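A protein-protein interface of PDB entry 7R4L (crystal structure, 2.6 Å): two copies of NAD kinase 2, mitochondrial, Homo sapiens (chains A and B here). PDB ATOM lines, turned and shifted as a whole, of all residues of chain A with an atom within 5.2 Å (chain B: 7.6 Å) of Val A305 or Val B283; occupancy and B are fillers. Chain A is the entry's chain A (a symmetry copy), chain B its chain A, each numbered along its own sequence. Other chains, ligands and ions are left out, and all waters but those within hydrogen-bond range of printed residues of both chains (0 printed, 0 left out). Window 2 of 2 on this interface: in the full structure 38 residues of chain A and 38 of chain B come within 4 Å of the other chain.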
ATOM      1  N   VAL A 280     -30.077 -15.105  13.837  1.00  0.00           N
ATOM      2  CA  VAL A 280     -29.491 -15.921  14.899  1.00  0.00           C
ATOM      3  C   VAL A 280     -28.403 -15.168  15.651  1.00  0.00           C
ATOM      4  O   VAL A 280     -28.245 -15.362  16.859  1.00  0.00           O
ATOM      5  CB  VAL A 280     -29.055 -17.313  14.407  1.00  0.00           C
ATOM      6  CG1 VAL A 280     -29.475 -17.483  12.999  1.00  0.00           C
ATOM      7  CG2 VAL A 280     -27.549 -17.528  14.557  1.00  0.00           C
ATOM      8  N   VAL A 283     -30.584 -13.525  18.060  1.00  0.00           N
ATOM      9  CA  VAL A 283     -31.169 -14.480  19.003  1.00  0.00           C
ATOM     10  C   VAL A 283     -30.132 -14.973  20.000  1.00  0.00           C
ATOM     11  O   VAL A 283     -30.421 -15.135  21.195  1.00  0.00           O
ATOM     12  CB  VAL A 283     -31.841 -15.642  18.246  1.00  0.00           C
ATOM     13  CG1 VAL A 283     -31.992 -16.861  19.151  1.00  0.00           C
ATOM     14  CG2 VAL A 283     -33.198 -15.203  17.701  1.00  0.00           C
ATOM     15  N   LEU A 284     -28.908 -15.219  19.531  1.00  0.00           N
ATOM     16  CA  LEU A 284     -27.832 -15.639  20.419  1.00  0.00           C
ATOM     17  C   LEU A 284     -27.329 -14.503  21.299  1.00  0.00           C
ATOM     18  O   LEU A 284     -26.618 -14.758  22.280  1.00  0.00           O
ATOM     19  CB  LEU A 284     -26.682 -16.219  19.593  1.00  0.00           C
ATOM     20  CG  LEU A 284     -26.969 -17.579  18.948  1.00  0.00           C
ATOM     21  CD1 LEU A 284     -25.741 -18.091  18.199  1.00  0.00           C
ATOM     22  CD2 LEU A 284     -27.462 -18.589  19.988  1.00  0.00           C
ATOM     23  N   GLU A 300     -17.882 -17.501  12.933  1.00  0.00           N
ATOM     24  CA  GLU A 300     -17.793 -18.956  12.974  1.00  0.00           C
ATOM     25  C   GLU A 300     -19.045 -19.567  13.598  1.00  0.00           C
ATOM     26  O   GLU A 300     -19.792 -20.299  12.938  1.00  0.00           O
ATOM     27  CB  GLU A 300     -16.533 -19.381  13.735  1.00  0.00           C
ATOM     28  N   LEU A 301     -19.300 -19.260  14.872  1.00  0.00           N
ATOM     29  CA  LEU A 301     -20.380 -19.934  15.583  1.00  0.00           C
ATOM     30  C   LEU A 301     -21.736 -19.603  14.976  1.00  0.00           C
ATOM     31  O   LEU A 301     -22.608 -20.475  14.873  1.00  0.00           O
ATOM     32  CB  LEU A 301     -20.356 -19.561  17.063  1.00  0.00           C
ATOM     33  CG  LEU A 301     -21.705 -19.729  17.766  1.00  0.00           C
ATOM     34  CD1 LEU A 301     -21.915 -21.186  18.178  1.00  0.00           C
ATOM     35  CD2 LEU A 301     -21.822 -18.810  18.958  1.00  0.00           C
ATOM     36  N   VAL A 302     -21.932 -18.353  14.564  1.00  0.00           N
ATOM     37  CA  VAL A 302     -23.210 -17.968  13.976  1.00  0.00           C
ATOM     38  C   VAL A 302     -23.475 -18.766  12.703  1.00  0.00           C
ATOM     39  O   VAL A 302     -24.568 -19.312  12.513  1.00  0.00           O
ATOM     40  CB  VAL A 302     -23.273 -16.443  13.760  1.00  0.00           C
ATOM     41  CG1 VAL A 302     -24.523 -16.057  12.984  1.00  0.00           C
ATOM     42  CG2 VAL A 302     -23.240 -15.727  15.104  1.00  0.00           C
ATOM     43  N   GLU A 303     -22.467 -18.884  11.832  1.00  0.00           N
ATOM     44  CA  GLU A 303     -22.631 -19.679  10.613  1.00  0.00           C
ATOM     45  C   GLU A 303     -22.860 -21.158  10.911  1.00  0.00           C
ATOM     46  O   GLU A 303     -23.615 -21.830  10.200  1.00  0.00           O
ATOM     47  CB  GLU A 303     -21.451 -19.478   9.658  1.00  0.00           C
ATOM     48  CG  GLU A 303     -21.629 -18.362   8.624  1.00  0.00           C
ATOM     49  CD  GLU A 303     -21.519 -16.956   9.194  1.00  0.00           C
ATOM     50  OE1 GLU A 303     -21.853 -16.735  10.377  1.00  0.00           O
ATOM     51  OE2 GLU A 303     -21.118 -16.053   8.434  1.00  0.00           O
ATOM     52  N   LYS A 304     -22.213 -21.687  11.949  1.00  0.00           N
ATOM     53  CA  LYS A 304     -22.431 -23.088  12.296  1.00  0.00           C
ATOM     54  C   LYS A 304     -23.874 -23.324  12.726  1.00  0.00           C
ATOM     55  O   LYS A 304     -24.521 -24.275  12.267  1.00  0.00           O
ATOM     56  CB  LYS A 304     -21.438 -23.553  13.371  1.00  0.00           C
ATOM     57  N   VAL A 305     -24.409 -22.449  13.579  1.00  0.00           N
ATOM     58  CA  VAL A 305     -25.751 -22.680  14.104  1.00  0.00           C
ATOM     59  C   VAL A 305     -26.816 -22.372  13.051  1.00  0.00           C
ATOM     60  O   VAL A 305     -27.847 -23.051  12.994  1.00  0.00           O
ATOM     61  CB  VAL A 305     -25.981 -21.934  15.434  1.00  0.00           C
ATOM     62  CG1 VAL A 305     -25.550 -20.491  15.322  1.00  0.00           C
ATOM     63  CG2 VAL A 305     -27.430 -22.049  15.899  1.00  0.00           C
ATOM     64  N   THR A 306     -26.587 -21.375  12.193  1.00  0.00           N
ATOM     65  CA  THR A 306     -27.526 -21.106  11.107  1.00  0.00           C
ATOM     66  C   THR A 306     -27.684 -22.325  10.208  1.00  0.00           C
ATOM     67  O   THR A 306     -28.804 -22.715   9.860  1.00  0.00           O
ATOM     68  CB  THR A 306     -27.027 -19.937  10.263  1.00  0.00           C
ATOM     69  OG1 THR A 306     -25.645 -20.148   9.953  1.00  0.00           O
ATOM     70  CG2 THR A 306     -27.151 -18.645  10.997  1.00  0.00           C
ATOM     71  N   ASN A 307     -26.562 -22.929   9.806  1.00  0.00           N
ATOM     72  CA  ASN A 307     -26.614 -24.021   8.841  1.00  0.00           C
ATOM     73  C   ASN A 307     -27.148 -25.304   9.448  1.00  0.00           C
ATOM     74  O   ASN A 307     -27.800 -26.083   8.749  1.00  0.00           O
ATOM     75  CB  ASN A 307     -25.253 -24.245   8.187  1.00  0.00           C
ATOM     76  CG  ASN A 307     -24.716 -22.995   7.536  1.00  0.00           C
ATOM     77  OD1 ASN A 307     -25.164 -21.892   7.830  1.00  0.00           O
ATOM     78  ND2 ASN A 307     -23.749 -23.159   6.640  1.00  0.00           N
ATOM     79  N   GLU A 308     -26.891 -25.560  10.726  1.00  0.00           N
ATOM     80  CA  GLU A 308     -27.570 -26.689  11.344  1.00  0.00           C
ATOM     81  C   GLU A 308     -29.073 -26.465  11.344  1.00  0.00           C
ATOM     82  O   GLU A 308     -29.839 -27.338  10.921  1.00  0.00           O
ATOM     83  CB  GLU A 308     -27.042 -26.969  12.748  1.00  0.00           C
ATOM     84  CG  GLU A 308     -26.836 -28.455  13.003  1.00  0.00           C
ATOM     85  CD  GLU A 308     -26.510 -28.767  14.442  1.00  0.00           C
ATOM     86  OE1 GLU A 308     -25.402 -28.410  14.877  1.00  0.00           O
ATOM     87  OE2 GLU A 308     -27.354 -29.372  15.132  1.00  0.00           O
ATOM     88  N   TYR A 309     -29.517 -25.280  11.780  1.00  0.00           N
ATOM     89  CA  TYR A 309     -30.951 -25.014  11.777  1.00  0.00           C
ATOM     90  C   TYR A 309     -31.532 -25.171  10.384  1.00  0.00           C
ATOM     91  O   TYR A 309     -32.594 -25.779  10.213  1.00  0.00           O
ATOM     92  CB  TYR A 309     -31.292 -23.628  12.311  1.00  0.00           C
ATOM     93  CG  TYR A 309     -32.792 -23.480  12.364  1.00  0.00           C
ATOM     94  CD1 TYR A 309     -33.512 -23.997  13.430  1.00  0.00           C
ATOM     95  CD2 TYR A 309     -33.503 -22.903  11.313  1.00  0.00           C
ATOM     96  CE1 TYR A 309     -34.886 -23.901  13.477  1.00  0.00           C
ATOM     97  CE2 TYR A 309     -34.871 -22.810  11.351  1.00  0.00           C
ATOM     98  CZ  TYR A 309     -35.559 -23.313  12.437  1.00  0.00           C
ATOM     99  OH  TYR A 309     -36.929 -23.230  12.491  1.00  0.00           O
ATOM    100  N   ASN A 310     -30.847 -24.633   9.376  1.00  0.00           N
ATOM    101  CA  ASN A 310     -31.424 -24.611   8.040  1.00  0.00           C
ATOM    102  C   ASN A 310     -31.403 -25.988   7.401  1.00  0.00           C
ATOM    103  O   ASN A 310     -32.352 -26.362   6.695  1.00  0.00           O
ATOM    104  CB  ASN A 310     -30.742 -23.559   7.182  1.00  0.00           C
ATOM    105  CG  ASN A 310     -31.195 -22.162   7.546  1.00  0.00           C
ATOM    106  OD1 ASN A 310     -32.298 -21.981   8.068  1.00  0.00           O
ATOM    107  ND2 ASN A 310     -30.347 -21.169   7.289  1.00  0.00           N
ATOM    108  N   VAL B 275     -40.121 -14.594  14.439  1.00  0.00           N
ATOM    109  CA  VAL B 275     -39.546 -15.918  14.591  1.00  0.00           C
ATOM    110  C   VAL B 275     -40.452 -16.726  15.504  1.00  0.00           C
ATOM    111  O   VAL B 275     -40.928 -16.215  16.526  1.00  0.00           O
ATOM    112  CB  VAL B 275     -38.122 -15.821  15.152  1.00  0.00           C
ATOM    113  CG1 VAL B 275     -37.789 -17.051  15.922  1.00  0.00           C
ATOM    114  CG2 VAL B 275     -37.134 -15.633  14.020  1.00  0.00           C
ATOM    115  N   THR B 277     -41.648 -19.495  18.219  1.00  0.00           N
ATOM    116  CA  THR B 277     -41.050 -19.897  19.485  1.00  0.00           C
ATOM    117  C   THR B 277     -40.369 -21.264  19.371  1.00  0.00           C
ATOM    118  O   THR B 277     -39.372 -21.525  20.057  1.00  0.00           O
ATOM    119  CB  THR B 277     -42.083 -19.789  20.623  1.00  0.00           C
ATOM    120  OG1 THR B 277     -41.491 -20.163  21.873  1.00  0.00           O
ATOM    121  CG2 THR B 277     -43.288 -20.678  20.357  1.00  0.00           C
ATOM    122  N   GLN B 278     -40.840 -22.125  18.467  1.00  0.00           N
ATOM    123  CA  GLN B 278     -40.146 -23.391  18.242  1.00  0.00           C
ATOM    124  C   GLN B 278     -38.802 -23.176  17.552  1.00  0.00           C
ATOM    125  O   GLN B 278     -37.813 -23.839  17.889  1.00  0.00           O
ATOM    126  CB  GLN B 278     -41.019 -24.352  17.432  1.00  0.00           C
ATOM    127  CG  GLN B 278     -40.309 -25.646  17.063  1.00  0.00           C
ATOM    128  CD  GLN B 278     -39.911 -26.465  18.293  1.00  0.00           C
ATOM    129  OE1 GLN B 278     -40.614 -26.480  19.306  1.00  0.00           O
ATOM    130  NE2 GLN B 278     -38.771 -27.135  18.209  1.00  0.00           N
ATOM    131  N   ALA B 279     -38.743 -22.252  16.587  1.00  0.00           N
ATOM    132  CA  ALA B 279     -37.486 -21.997  15.890  1.00  0.00           C
ATOM    133  C   ALA B 279     -36.382 -21.570  16.846  1.00  0.00           C
ATOM    134  O   ALA B 279     -35.215 -21.899  16.619  1.00  0.00           O
ATOM    135  CB  ALA B 279     -37.677 -20.965  14.776  1.00  0.00           C
ATOM    136  N   VAL B 280     -36.717 -20.849  17.919  1.00  0.00           N
ATOM    137  CA  VAL B 280     -35.675 -20.481  18.875  1.00  0.00           C
ATOM    138  C   VAL B 280     -35.375 -21.616  19.844  1.00  0.00           C
ATOM    139  O   VAL B 280     -34.225 -21.782  20.257  1.00  0.00           O
ATOM    140  CB  VAL B 280     -35.951 -19.133  19.565  1.00  0.00           C
ATOM    141  CG1 VAL B 280     -37.152 -18.517  18.963  1.00  0.00           C
ATOM    142  CG2 VAL B 280     -36.116 -19.288  21.077  1.00  0.00           C
ATOM    143  N   GLU B 281     -36.379 -22.418  20.210  1.00  0.00           N
ATOM    144  CA  GLU B 281     -36.098 -23.667  20.911  1.00  0.00           C
ATOM    145  C   GLU B 281     -35.039 -24.474  20.176  1.00  0.00           C
ATOM    146  O   GLU B 281     -34.046 -24.902  20.769  1.00  0.00           O
ATOM    147  CB  GLU B 281     -37.371 -24.496  21.078  1.00  0.00           C
ATOM    148  CG  GLU B 281     -37.726 -24.788  22.527  1.00  0.00           C
ATOM    149  CD  GLU B 281     -38.957 -25.666  22.666  1.00  0.00           C
ATOM    150  OE1 GLU B 281     -38.869 -26.887  22.391  1.00  0.00           O
ATOM    151  OE2 GLU B 281     -40.020 -25.122  23.040  1.00  0.00           O
ATOM    152  N   ASP B 282     -35.231 -24.676  18.873  1.00  0.00           N
ATOM    153  CA  ASP B 282     -34.226 -25.378  18.079  1.00  0.00           C
ATOM    154  C   ASP B 282     -32.898 -24.629  18.096  1.00  0.00           C
ATOM    155  O   ASP B 282     -31.857 -25.204  18.429  1.00  0.00           O
ATOM    156  CB  ASP B 282     -34.720 -25.581  16.642  1.00  0.00           C
ATOM    157  CG  ASP B 282     -35.991 -26.424  16.568  1.00  0.00           C
ATOM    158  OD1 ASP B 282     -36.678 -26.538  17.604  1.00  0.00           O
ATOM    159  OD2 ASP B 282     -36.308 -26.961  15.477  1.00  0.00           O
ATOM    160  N   VAL B 283     -32.924 -23.334  17.770  1.00  0.00           N
ATOM    161  CA  VAL B 283     -31.690 -22.557  17.631  1.00  0.00           C
ATOM    162  C   VAL B 283     -30.884 -22.571  18.919  1.00  0.00           C
ATOM    163  O   VAL B 283     -29.648 -22.670  18.899  1.00  0.00           O
ATOM    164  CB  VAL B 283     -32.007 -21.123  17.162  1.00  0.00           C
ATOM    165  CG1 VAL B 283     -30.856 -20.179  17.498  1.00  0.00           C
ATOM    166  CG2 VAL B 283     -32.298 -21.108  15.664  1.00  0.00           C
ATOM    167  N   LEU B 284     -31.564 -22.476  20.063  1.00  0.00           N
ATOM    168  CA  LEU B 284     -30.885 -22.538  21.351  1.00  0.00           C
ATOM    169  C   LEU B 284     -30.407 -23.944  21.686  1.00  0.00           C
ATOM    170  O   LEU B 284     -29.589 -24.109  22.600  1.00  0.00           O
ATOM    171  CB  LEU B 284     -31.816 -22.018  22.447  1.00  0.00           C
ATOM    172  CG  LEU B 284     -32.074 -20.508  22.416  1.00  0.00           C
ATOM    173  CD1 LEU B 284     -32.966 -20.089  23.583  1.00  0.00           C
ATOM    174  CD2 LEU B 284     -30.759 -19.724  22.396  1.00  0.00           C
ATOM    175  N   ASN B 285     -30.888 -24.957  20.972  1.00  0.00           N
ATOM    176  CA  ASN B 285     -30.422 -26.312  21.201  1.00  0.00           C
ATOM    177  C   ASN B 285     -29.182 -26.627  20.374  1.00  0.00           C
ATOM    178  O   ASN B 285     -28.284 -27.314  20.865  1.00  0.00           O
ATOM    179  CB  ASN B 285     -31.550 -27.307  20.930  1.00  0.00           C
ATOM    180  CG  ASN B 285     -32.279 -27.719  22.198  1.00  0.00           C
ATOM    181  OD1 ASN B 285     -31.667 -27.883  23.247  1.00  0.00           O
ATOM    182  ND2 ASN B 285     -33.598 -27.869  22.107  1.00  0.00           N
ATOM    183  N   ILE B 286     -29.098 -26.137  19.130  1.00  0.00           N
ATOM    184  CA  ILE B 286     -27.810 -26.180  18.437  1.00  0.00           C
ATOM    185  C   ILE B 286     -26.750 -25.461  19.255  1.00  0.00           C
ATOM    186  O   ILE B 286     -25.569 -25.830  19.225  1.00  0.00           O
ATOM    187  CB  ILE B 286     -27.860 -25.667  16.972  1.00  0.00           C
ATOM    188  CG1 ILE B 286     -28.895 -26.402  16.108  1.00  0.00           C
ATOM    189  CG2 ILE B 286     -26.482 -25.741  16.314  1.00  0.00           C
ATOM    190  CD1 ILE B 286     -30.219 -25.697  15.966  1.00  0.00           C
ATOM    191  N   ALA B 287     -27.159 -24.453  20.028  1.00  0.00           N
ATOM    192  CA  ALA B 287     -26.210 -23.649  20.792  1.00  0.00           C
ATOM    193  C   ALA B 287     -25.514 -24.479  21.866  1.00  0.00           C
ATOM    194  O   ALA B 287     -24.280 -24.501  21.949  1.00  0.00           O
ATOM    195  CB  ALA B 287     -26.925 -22.443  21.403  1.00  0.00           C
ATOM    196  N   LYS B 288     -26.287 -25.169  22.707  1.00  0.00           N
ATOM    197  CA  LYS B 288     -25.656 -25.953  23.761  1.00  0.00           C
ATOM    198  C   LYS B 288     -24.893 -27.142  23.192  1.00  0.00           C
ATOM    199  O   LYS B 288     -23.855 -27.529  23.742  1.00  0.00           O
ATOM    200  CB  LYS B 288     -26.680 -26.397  24.807  1.00  0.00           C
ATOM    201  N   ARG B 289     -25.374 -27.724  22.093  1.00  0.00           N
ATOM    202  CA  ARG B 289     -24.669 -28.825  21.450  1.00  0.00           C
ATOM    203  C   ARG B 289     -23.418 -28.310  20.752  1.00  0.00           C
ATOM    204  O   ARG B 289     -22.297 -28.563  21.207  1.00  0.00           O
ATOM    205  CB  ARG B 289     -25.577 -29.548  20.451  1.00  0.00           C
ATOM    206  N   GLN B 290     -23.597 -27.573  19.659  1.00  0.00           N
ATOM    207  CA  GLN B 290     -22.465 -27.033  18.917  1.00  0.00           C
ATOM    208  C   GLN B 290     -21.788 -25.909  19.695  1.00  0.00           C
ATOM    209  O   GLN B 290     -21.607 -24.808  19.164  1.00  0.00           O
ATOM    210  CB  GLN B 290     -22.916 -26.532  17.541  1.00  0.00           C
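Among the printed residues, pairs that only touch across the chains: Val A283 with Val B283 (3.9 Å), Leu A301 with Gln B290 (3.8 Å), Val A305 with Val B283 (3.8 Å), Val A305 with Ile B286 (3.8 Å), Glu A308 with Ile B286 (3.2 Å), Tyr A309 with Ala B279 (3.3 Å), Tyr A309 with Asp B282 (3.6 Å) and Tyr A309 with Val B283 (3.8 Å).
Val A283 touches its own counterpart, Val B283.
Positions printed for both chains: 280, 283 and 284.
Of the 8 pairs that touch across the chains among the printed residues, 1 has its exchanged pair printed and touching as well.
Of chain B, only Val B283 and Ile B286 come within 4 Å of Val A305.
Printed residues of chain A within 4 Å of Val B283: Val A283 (3.9 Å), Val A305 (3.8 Å) and Tyr A309 (3.8 Å).
No residue of chain B comes within 4 Å of Lys A304.
Of the printed residues of chain B, Leu A301 touches Gln B290.
Printed residues of chain B within 4 Å of Tyr A309: Ala B279, Asp B282 and Val B283.
Of the printed residues of chain B, Glu A308 touches Ile B286 (3.2 Å).
Lys B288 touches none of the printed residues of chain A.
Glu B281 touches none of the printed residues of chain A.
The nearest residue of chain B that does not touch Val A305 is Ala B287 (4.8 Å).
Of the 14 printed residues of chain A, 5 touch a printed residue of chain B.
Hydrophobic or aromatic side chains of chain A within 4 Å of the printed part of chain B: Val A283, Leu A301, Val A305 and Tyr A309.
Along chain A the printed residues that touch a printed residue of chain B span positions 283 to 309.
Among the printed residues, no Asp or Glu carboxylate lies within 4 Å of a Lys or Arg side-chain nitrogen of the other chain.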
